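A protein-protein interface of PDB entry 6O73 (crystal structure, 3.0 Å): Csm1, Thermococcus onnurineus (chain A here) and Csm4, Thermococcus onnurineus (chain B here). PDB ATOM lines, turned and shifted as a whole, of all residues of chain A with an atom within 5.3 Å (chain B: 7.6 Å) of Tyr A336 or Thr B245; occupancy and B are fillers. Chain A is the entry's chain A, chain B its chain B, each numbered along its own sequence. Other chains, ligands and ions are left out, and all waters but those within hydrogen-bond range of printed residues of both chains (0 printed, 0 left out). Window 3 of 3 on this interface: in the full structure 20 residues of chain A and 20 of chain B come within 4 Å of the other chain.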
ATOM      1  N   VAL A 332      18.987 -23.442 -36.051  1.00  0.00           N
ATOM      2  CA  VAL A 332      18.560 -23.433 -34.620  1.00  0.00           C
ATOM      3  C   VAL A 332      18.205 -21.995 -34.232  1.00  0.00           C
ATOM      4  O   VAL A 332      17.085 -21.783 -33.745  1.00  0.00           O
ATOM      5  CB  VAL A 332      19.629 -24.017 -33.680  1.00  0.00           C
ATOM      6  CG1 VAL A 332      19.346 -23.661 -32.228  1.00  0.00           C
ATOM      7  CG2 VAL A 332      19.745 -25.524 -33.841  1.00  0.00           C
ATOM      8  N   GLU A 333      19.133 -21.056 -34.437  1.00  0.00           N
ATOM      9  CA  GLU A 333      18.942 -19.610 -34.146  1.00  0.00           C
ATOM     10  C   GLU A 333      17.643 -19.131 -34.785  1.00  0.00           C
ATOM     11  O   GLU A 333      16.767 -18.666 -34.043  1.00  0.00           O
ATOM     12  CB  GLU A 333      20.101 -18.772 -34.675  1.00  0.00           C
ATOM     13  CG  GLU A 333      21.357 -18.920 -33.847  1.00  0.00           C
ATOM     14  CD  GLU A 333      22.636 -18.870 -34.661  1.00  0.00           C
ATOM     15  OE1 GLU A 333      22.682 -18.094 -35.638  1.00  0.00           O
ATOM     16  OE2 GLU A 333      23.578 -19.618 -34.328  1.00  0.00           O
ATOM     17  N   TRP A 334      17.515 -19.259 -36.103  1.00  0.00           N
ATOM     18  CA  TRP A 334      16.297 -18.807 -36.819  1.00  0.00           C
ATOM     19  C   TRP A 334      15.052 -19.358 -36.111  1.00  0.00           C
ATOM     20  O   TRP A 334      14.036 -18.638 -36.081  1.00  0.00           O
ATOM     21  CB  TRP A 334      16.326 -19.198 -38.296  1.00  0.00           C
ATOM     22  CG  TRP A 334      15.095 -18.732 -39.007  1.00  0.00           C
ATOM     23  CD1 TRP A 334      14.909 -17.532 -39.629  1.00  0.00           C
ATOM     24  CD2 TRP A 334      13.855 -19.447 -39.133  1.00  0.00           C
ATOM     25  NE1 TRP A 334      13.646 -17.460 -40.155  1.00  0.00           N
ATOM     26  CE2 TRP A 334      12.976 -18.620 -39.864  1.00  0.00           C
ATOM     27  CE3 TRP A 334      13.410 -20.707 -38.717  1.00  0.00           C
ATOM     28  CZ2 TRP A 334      11.678 -19.013 -40.183  1.00  0.00           C
ATOM     29  CZ3 TRP A 334      12.127 -21.094 -39.030  1.00  0.00           C
ATOM     30  CH2 TRP A 334      11.274 -20.256 -39.753  1.00  0.00           C
ATOM     31  N   LEU A 335      15.126 -20.579 -35.568  1.00  0.00           N
ATOM     32  CA  LEU A 335      13.996 -21.225 -34.845  1.00  0.00           C
ATOM     33  C   LEU A 335      13.790 -20.556 -33.483  1.00  0.00           C
ATOM     34  O   LEU A 335      12.631 -20.535 -33.012  1.00  0.00           O
ATOM     35  CB  LEU A 335      14.254 -22.726 -34.678  1.00  0.00           C
ATOM     36  CG  LEU A 335      13.734 -23.615 -35.804  1.00  0.00           C
ATOM     37  CD1 LEU A 335      14.179 -25.050 -35.583  1.00  0.00           C
ATOM     38  CD2 LEU A 335      12.216 -23.542 -35.920  1.00  0.00           C
ATOM     39  N   TYR A 336      14.859 -20.049 -32.864  1.00  0.00           N
ATOM     40  CA  TYR A 336      14.799 -19.416 -31.521  1.00  0.00           C
ATOM     41  C   TYR A 336      14.189 -18.012 -31.631  1.00  0.00           C
ATOM     42  O   TYR A 336      13.336 -17.666 -30.791  1.00  0.00           O
ATOM     43  CB  TYR A 336      16.167 -19.370 -30.834  1.00  0.00           C
ATOM     44  CG  TYR A 336      16.061 -18.912 -29.403  1.00  0.00           C
ATOM     45  CD1 TYR A 336      16.045 -17.562 -29.087  1.00  0.00           C
ATOM     46  CD2 TYR A 336      15.892 -19.821 -28.369  1.00  0.00           C
ATOM     47  CE1 TYR A 336      15.905 -17.128 -27.779  1.00  0.00           C
ATOM     48  CE2 TYR A 336      15.753 -19.404 -27.056  1.00  0.00           C
ATOM     49  CZ  TYR A 336      15.760 -18.052 -26.760  1.00  0.00           C
ATOM     50  OH  TYR A 336      15.622 -17.631 -25.469  1.00  0.00           O
ATOM     51  N   ARG A 337      14.615 -17.228 -32.625  1.00  0.00           N
ATOM     52  CA  ARG A 337      14.184 -15.816 -32.800  1.00  0.00           C
ATOM     53  C   ARG A 337      12.695 -15.789 -33.138  1.00  0.00           C
ATOM     54  O   ARG A 337      11.996 -14.883 -32.648  1.00  0.00           O
ATOM     55  CB  ARG A 337      14.962 -15.123 -33.920  1.00  0.00           C
ATOM     56  CG  ARG A 337      16.472 -15.208 -33.780  1.00  0.00           C
ATOM     57  CD  ARG A 337      17.125 -14.585 -34.990  1.00  0.00           C
ATOM     58  NE  ARG A 337      18.568 -14.502 -34.840  1.00  0.00           N
ATOM     59  CZ  ARG A 337      19.347 -13.634 -35.478  1.00  0.00           C
ATOM     60  NH1 ARG A 337      18.827 -12.755 -36.320  1.00  0.00           N
ATOM     61  NH2 ARG A 337      20.652 -13.644 -35.264  1.00  0.00           N
ATOM     62  N   GLU A 338      12.243 -16.748 -33.948  1.00  0.00           N
ATOM     63  CA  GLU A 338      10.889 -16.748 -34.558  1.00  0.00           C
ATOM     64  C   GLU A 338       9.883 -17.426 -33.615  1.00  0.00           C
ATOM     65  O   GLU A 338       8.701 -17.031 -33.676  1.00  0.00           O
ATOM     66  CB  GLU A 338      10.936 -17.402 -35.943  1.00  0.00           C
ATOM     67  CG  GLU A 338       9.608 -17.370 -36.685  1.00  0.00           C
ATOM     68  CD  GLU A 338       9.114 -15.993 -37.098  1.00  0.00           C
ATOM     69  OE1 GLU A 338       7.907 -15.718 -36.920  1.00  0.00           O
ATOM     70  OE2 GLU A 338       9.935 -15.202 -37.612  1.00  0.00           O
ATOM     71  N   PHE A 339      10.302 -18.382 -32.774  1.00  0.00           N
ATOM     72  CA  PHE A 339       9.363 -19.194 -31.949  1.00  0.00           C
ATOM     73  C   PHE A 339       9.813 -19.342 -30.490  1.00  0.00           C
ATOM     74  O   PHE A 339       9.158 -20.112 -29.761  1.00  0.00           O
ATOM     75  CB  PHE A 339       9.162 -20.565 -32.598  1.00  0.00           C
ATOM     76  CG  PHE A 339       8.628 -20.478 -34.002  1.00  0.00           C
ATOM     77  CD1 PHE A 339       7.402 -19.879 -34.246  1.00  0.00           C
ATOM     78  CD2 PHE A 339       9.362 -20.954 -35.075  1.00  0.00           C
ATOM     79  CE1 PHE A 339       6.913 -19.774 -35.539  1.00  0.00           C
ATOM     80  CE2 PHE A 339       8.869 -20.854 -36.366  1.00  0.00           C
ATOM     81  CZ  PHE A 339       7.647 -20.265 -36.593  1.00  0.00           C
ATOM     82  N   GLU A 340      10.844 -18.620 -30.047  1.00  0.00           N
ATOM     83  CA  GLU A 340      11.447 -18.850 -28.706  1.00  0.00           C
ATOM     84  C   GLU A 340      11.828 -20.335 -28.648  1.00  0.00           C
ATOM     85  O   GLU A 340      12.166 -20.886 -29.713  1.00  0.00           O
ATOM     86  CB  GLU A 340      10.469 -18.444 -27.598  1.00  0.00           C
ATOM     87  CG  GLU A 340       9.820 -17.085 -27.809  1.00  0.00           C
ATOM     88  CD  GLU A 340       8.794 -16.711 -26.751  1.00  0.00           C
ATOM     89  OE1 GLU A 340       8.029 -17.603 -26.330  1.00  0.00           O
ATOM     90  OE2 GLU A 340       8.766 -15.532 -26.345  1.00  0.00           O
ATOM     91  N   SER A 341      11.739 -20.982 -27.484  1.00  0.00           N
ATOM     92  CA  SER A 341      12.141 -22.402 -27.314  1.00  0.00           C
ATOM     93  C   SER A 341      11.028 -23.365 -27.752  1.00  0.00           C
ATOM     94  O   SER A 341      11.217 -24.583 -27.562  1.00  0.00           O
ATOM     95  CB  SER A 341      12.565 -22.675 -25.897  1.00  0.00           C
ATOM     96  OG  SER A 341      12.659 -24.073 -25.663  1.00  0.00           O
ATOM     97  N   PHE A 385      18.763 -25.787 -27.878  1.00  0.00           N
ATOM     98  CA  PHE A 385      19.321 -24.442 -28.157  1.00  0.00           C
ATOM     99  C   PHE A 385      20.623 -24.234 -27.384  1.00  0.00           C
ATOM    100  O   PHE A 385      20.976 -23.063 -27.149  1.00  0.00           O
ATOM    101  CB  PHE A 385      18.304 -23.363 -27.787  1.00  0.00           C
ATOM    102  CG  PHE A 385      17.003 -23.493 -28.527  1.00  0.00           C
ATOM    103  CD1 PHE A 385      16.892 -23.050 -29.835  1.00  0.00           C
ATOM    104  CD2 PHE A 385      15.903 -24.085 -27.929  1.00  0.00           C
ATOM    105  CE1 PHE A 385      15.699 -23.178 -30.524  1.00  0.00           C
ATOM    106  CE2 PHE A 385      14.711 -24.217 -28.622  1.00  0.00           C
ATOM    107  CZ  PHE A 385      14.611 -23.759 -29.916  1.00  0.00           C
ATOM    108  N   ILE A 388      23.088 -21.900 -29.013  1.00  0.00           N
ATOM    109  CA  ILE A 388      22.833 -20.437 -28.860  1.00  0.00           C
ATOM    110  C   ILE A 388      23.381 -20.014 -27.497  1.00  0.00           C
ATOM    111  O   ILE A 388      22.726 -20.320 -26.481  1.00  0.00           O
ATOM    112  CB  ILE A 388      21.329 -20.144 -29.003  1.00  0.00           C
ATOM    113  CG1 ILE A 388      20.858 -20.360 -30.441  1.00  0.00           C
ATOM    114  CG2 ILE A 388      20.979 -18.748 -28.501  1.00  0.00           C
ATOM    115  CD1 ILE A 388      19.359 -20.390 -30.589  1.00  0.00           C
ATOM    116  N   LEU A 391      21.673 -17.511 -24.888  1.00  0.00           N
ATOM    117  CA  LEU A 391      20.475 -18.100 -24.229  1.00  0.00           C
ATOM    118  C   LEU A 391      20.548 -17.894 -22.711  1.00  0.00           C
ATOM    119  O   LEU A 391      19.502 -17.569 -22.122  1.00  0.00           O
ATOM    120  CB  LEU A 391      20.364 -19.588 -24.574  1.00  0.00           C
ATOM    121  CG  LEU A 391      19.207 -20.326 -23.898  1.00  0.00           C
ATOM    122  CD1 LEU A 391      17.873 -19.655 -24.193  1.00  0.00           C
ATOM    123  CD2 LEU A 391      19.172 -21.784 -24.324  1.00  0.00           C
ATOM    124  N   ALA B 218      16.107 -23.340 -12.317  1.00  0.00           N
ATOM    125  CA  ALA B 218      17.263 -22.435 -12.131  1.00  0.00           C
ATOM    126  C   ALA B 218      17.434 -21.522 -13.347  1.00  0.00           C
ATOM    127  O   ALA B 218      16.971 -21.884 -14.444  1.00  0.00           O
ATOM    128  CB  ALA B 218      18.518 -23.235 -11.893  1.00  0.00           C
ATOM    129  N   LEU B 219      18.086 -20.378 -13.127  1.00  0.00           N
ATOM    130  CA  LEU B 219      18.677 -19.510 -14.178  1.00  0.00           C
ATOM    131  C   LEU B 219      20.178 -19.774 -14.191  1.00  0.00           C
ATOM    132  O   LEU B 219      20.886 -19.340 -13.286  1.00  0.00           O
ATOM    133  CB  LEU B 219      18.401 -18.038 -13.863  1.00  0.00           C
ATOM    134  CG  LEU B 219      16.972 -17.675 -13.469  1.00  0.00           C
ATOM    135  CD1 LEU B 219      16.957 -16.318 -12.791  1.00  0.00           C
ATOM    136  CD2 LEU B 219      16.041 -17.677 -14.669  1.00  0.00           C
ATOM    137  N   PRO B 220      20.706 -20.531 -15.178  1.00  0.00           N
ATOM    138  CA  PRO B 220      22.109 -20.946 -15.145  1.00  0.00           C
ATOM    139  C   PRO B 220      23.076 -19.795 -15.465  1.00  0.00           C
ATOM    140  O   PRO B 220      22.632 -18.804 -16.005  1.00  0.00           O
ATOM    141  CB  PRO B 220      22.163 -22.066 -16.195  1.00  0.00           C
ATOM    142  CG  PRO B 220      21.055 -21.721 -17.171  1.00  0.00           C
ATOM    143  CD  PRO B 220      19.978 -21.057 -16.343  1.00  0.00           C
ATOM    144  N   LEU B 229      14.354 -26.844 -21.314  1.00  0.00           N
ATOM    145  CA  LEU B 229      14.027 -25.410 -21.143  1.00  0.00           C
ATOM    146  C   LEU B 229      12.619 -25.280 -20.573  1.00  0.00           C
ATOM    147  O   LEU B 229      11.784 -26.168 -20.785  1.00  0.00           O
ATOM    148  CB  LEU B 229      14.125 -24.674 -22.478  1.00  0.00           C
ATOM    149  CG  LEU B 229      15.538 -24.460 -23.008  1.00  0.00           C
ATOM    150  CD1 LEU B 229      15.483 -23.863 -24.399  1.00  0.00           C
ATOM    151  CD2 LEU B 229      16.348 -23.569 -22.075  1.00  0.00           C
ATOM    152  N   LEU B 230      12.390 -24.159 -19.910  1.00  0.00           N
ATOM    153  CA  LEU B 230      11.132 -23.831 -19.212  1.00  0.00           C
ATOM    154  C   LEU B 230      10.886 -22.340 -19.420  1.00  0.00           C
ATOM    155  O   LEU B 230      11.762 -21.546 -19.043  1.00  0.00           O
ATOM    156  CB  LEU B 230      11.326 -24.189 -17.741  1.00  0.00           C
ATOM    157  CG  LEU B 230      10.054 -24.393 -16.933  1.00  0.00           C
ATOM    158  CD1 LEU B 230       9.465 -25.770 -17.191  1.00  0.00           C
ATOM    159  CD2 LEU B 230      10.343 -24.202 -15.456  1.00  0.00           C
ATOM    160  N   ARG B 231       9.764 -21.991 -20.050  1.00  0.00           N
ATOM    161  CA  ARG B 231       9.437 -20.599 -20.450  1.00  0.00           C
ATOM    162  C   ARG B 231       8.416 -20.014 -19.470  1.00  0.00           C
ATOM    163  O   ARG B 231       7.443 -20.721 -19.137  1.00  0.00           O
ATOM    164  CB  ARG B 231       8.885 -20.576 -21.876  1.00  0.00           C
ATOM    165  CG  ARG B 231       8.665 -19.175 -22.421  1.00  0.00           C
ATOM    166  CD  ARG B 231       9.977 -18.494 -22.748  1.00  0.00           C
ATOM    167  NE  ARG B 231       9.768 -17.116 -23.167  1.00  0.00           N
ATOM    168  CZ  ARG B 231      10.738 -16.256 -23.461  1.00  0.00           C
ATOM    169  NH1 ARG B 231      12.004 -16.631 -23.390  1.00  0.00           N
ATOM    170  NH2 ARG B 231      10.440 -15.023 -23.830  1.00  0.00           N
ATOM    171  N   LYS B 232       8.626 -18.762 -19.053  1.00  0.00           N
ATOM    172  CA  LYS B 232       7.763 -18.048 -18.075  1.00  0.00           C
ATOM    173  C   LYS B 232       7.726 -16.551 -18.400  1.00  0.00           C
ATOM    174  O   LYS B 232       7.047 -15.822 -17.645  1.00  0.00           O
ATOM    175  CB  LYS B 232       8.287 -18.291 -16.659  1.00  0.00           C
ATOM    176  CG  LYS B 232       7.930 -19.643 -16.063  1.00  0.00           C
ATOM    177  CD  LYS B 232       7.977 -19.618 -14.558  1.00  0.00           C
ATOM    178  CE  LYS B 232       7.365 -20.838 -13.915  1.00  0.00           C
ATOM    179  NZ  LYS B 232       7.283 -20.672 -12.446  1.00  0.00           N
ATOM    180  N   ARG B 243       9.327 -12.276 -18.756  1.00  0.00           N
ATOM    181  CA  ARG B 243       9.549 -13.600 -19.401  1.00  0.00           C
ATOM    182  C   ARG B 243      11.012 -14.020 -19.223  1.00  0.00           C
ATOM    183  O   ARG B 243      11.904 -13.252 -19.641  1.00  0.00           O
ATOM    184  CB  ARG B 243       9.196 -13.560 -20.890  1.00  0.00           C
ATOM    185  CG  ARG B 243       7.705 -13.445 -21.165  1.00  0.00           C
ATOM    186  CD  ARG B 243       7.336 -13.842 -22.581  1.00  0.00           C
ATOM    187  NE  ARG B 243       5.894 -13.987 -22.714  1.00  0.00           N
ATOM    188  CZ  ARG B 243       5.192 -15.050 -22.324  1.00  0.00           C
ATOM    189  NH1 ARG B 243       5.793 -16.093 -21.770  1.00  0.00           N
ATOM    190  NH2 ARG B 243       3.880 -15.066 -22.488  1.00  0.00           N
ATOM    191  N   MET B 244      11.226 -15.204 -18.640  1.00  0.00           N
ATOM    192  CA  MET B 244      12.559 -15.790 -18.346  1.00  0.00           C
ATOM    193  C   MET B 244      12.596 -17.217 -18.897  1.00  0.00           C
ATOM    194  O   MET B 244      11.580 -17.924 -18.760  1.00  0.00           O
ATOM    195  CB  MET B 244      12.805 -15.866 -16.836  1.00  0.00           C
ATOM    196  CG  MET B 244      12.451 -14.602 -16.084  1.00  0.00           C
ATOM    197  SD  MET B 244      13.594 -13.251 -16.437  1.00  0.00           S
ATOM    198  CE  MET B 244      15.168 -14.047 -16.123  1.00  0.00           C
ATOM    199  N   THR B 245      13.727 -17.623 -19.475  1.00  0.00           N
ATOM    200  CA  THR B 245      14.040 -19.045 -19.762  1.00  0.00           C
ATOM    201  C   THR B 245      14.713 -19.646 -18.528  1.00  0.00           C
ATOM    202  O   THR B 245      15.882 -19.299 -18.248  1.00  0.00           O
ATOM    203  CB  THR B 245      14.899 -19.221 -21.019  1.00  0.00           C
ATOM    204  OG1 THR B 245      16.054 -18.388 -20.924  1.00  0.00           O
ATOM    205  CG2 THR B 245      14.137 -18.889 -22.282  1.00  0.00           C
ATOM    206  N   PHE B 246      13.982 -20.497 -17.813  1.00  0.00           N
ATOM    207  CA  PHE B 246      14.530 -21.366 -16.749  1.00  0.00           C
ATOM    208  C   PHE B 246      14.982 -22.687 -17.363  1.00  0.00           C
ATOM    209  O   PHE B 246      14.586 -23.052 -18.490  1.00  0.00           O
ATOM    210  CB  PHE B 246      13.508 -21.640 -15.647  1.00  0.00           C
ATOM    211  CG  PHE B 246      13.256 -20.458 -14.752  1.00  0.00           C
ATOM    212  CD1 PHE B 246      13.875 -20.358 -13.518  1.00  0.00           C
ATOM    213  CD2 PHE B 246      12.417 -19.434 -15.161  1.00  0.00           C
ATOM    214  CE1 PHE B 246      13.647 -19.260 -12.706  1.00  0.00           C
ATOM    215  CE2 PHE B 246      12.192 -18.337 -14.350  1.00  0.00           C
ATOM    216  CZ  PHE B 246      12.806 -18.253 -13.124  1.00  0.00           C
ATOM    217  N   ILE B 247      15.831 -23.354 -16.595  1.00  0.00           N
ATOM    218  CA  ILE B 247      16.200 -24.783 -16.725  1.00  0.00           C
ATOM    219  C   ILE B 247      15.271 -25.554 -15.793  1.00  0.00           C
ATOM    220  O   ILE B 247      15.082 -25.083 -14.660  1.00  0.00           O
ATOM    221  CB  ILE B 247      17.687 -24.915 -16.363  1.00  0.00           C
ATOM    222  CG1 ILE B 247      18.542 -24.682 -17.606  1.00  0.00           C
ATOM    223  CG2 ILE B 247      17.999 -26.232 -15.679  1.00  0.00           C
ATOM    224  CD1 ILE B 247      19.957 -25.110 -17.434  1.00  0.00           C
ATOM    225  N   ALA B 248      14.694 -26.665 -16.249  1.00  0.00           N
ATOM    226  CA  ALA B 248      13.633 -27.391 -15.516  1.00  0.00           C
ATOM    227  C   ALA B 248      14.222 -28.101 -14.295  1.00  0.00           C
ATOM    228  O   ALA B 248      15.432 -28.398 -14.299  1.00  0.00           O
ATOM    229  CB  ALA B 248      12.948 -28.376 -16.424  1.00  0.00           C
ATOM    230  N   GLU B 261      17.913 -12.592 -10.019  1.00  0.00           N
ATOM    231  CA  GLU B 261      17.880 -11.430 -10.934  1.00  0.00           C
ATOM    232  C   GLU B 261      16.901 -10.395 -10.387  1.00  0.00           C
ATOM    233  O   GLU B 261      15.751 -10.756 -10.072  1.00  0.00           O
ATOM    234  CB  GLU B 261      17.607 -11.901 -12.360  1.00  0.00           C
ATOM    235  CG  GLU B 261      18.896 -12.282 -13.070  1.00  0.00           C
ATOM    236  CD  GLU B 261      18.756 -12.969 -14.417  1.00  0.00           C
ATOM    237  OE1 GLU B 261      17.865 -12.572 -15.193  1.00  0.00           O
ATOM    238  OE2 GLU B 261      19.552 -13.895 -14.692  1.00  0.00           O
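The side-chain carboxylate (OE2) of Glu A340 lies within salt-bridge range of the guanidinium group (NH2) of Arg B231 (3.1 Å).
Among the printed residues, pairs that only touch across the chains: Tyr A336 with Thr B245, Ser A341 with Leu B229, Phe A385 with Leu B229 and Leu A391 with Thr B245.
Tyr A336 touches just one residue of chain B: Thr B245.
Of the printed residues of chain B, Glu A340 touches Arg B231.
Of the printed residues of chain B, Ser A341 touches Leu B229.
Thr B245 touches just these residues of chain A: Tyr A336 and Leu A391.
The nearest residue of chain B that does not touch Tyr A336 is Arg B231 (4.3 Å).
Of the 13 printed residues of chain A, 5 touch a printed residue of chain B.
Of the 14 printed residues of chain B, 3 touch a printed residue of chain A.
Hydrophobic or aromatic side chains of chain B within 4 Å of the printed part of chain A: Leu B229.
Among the printed residues, Asp or Glu carboxylates within 4 Å of a Lys or Arg side-chain nitrogen of the other chain: Glu A340 with Arg B231 (3.1 Å).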
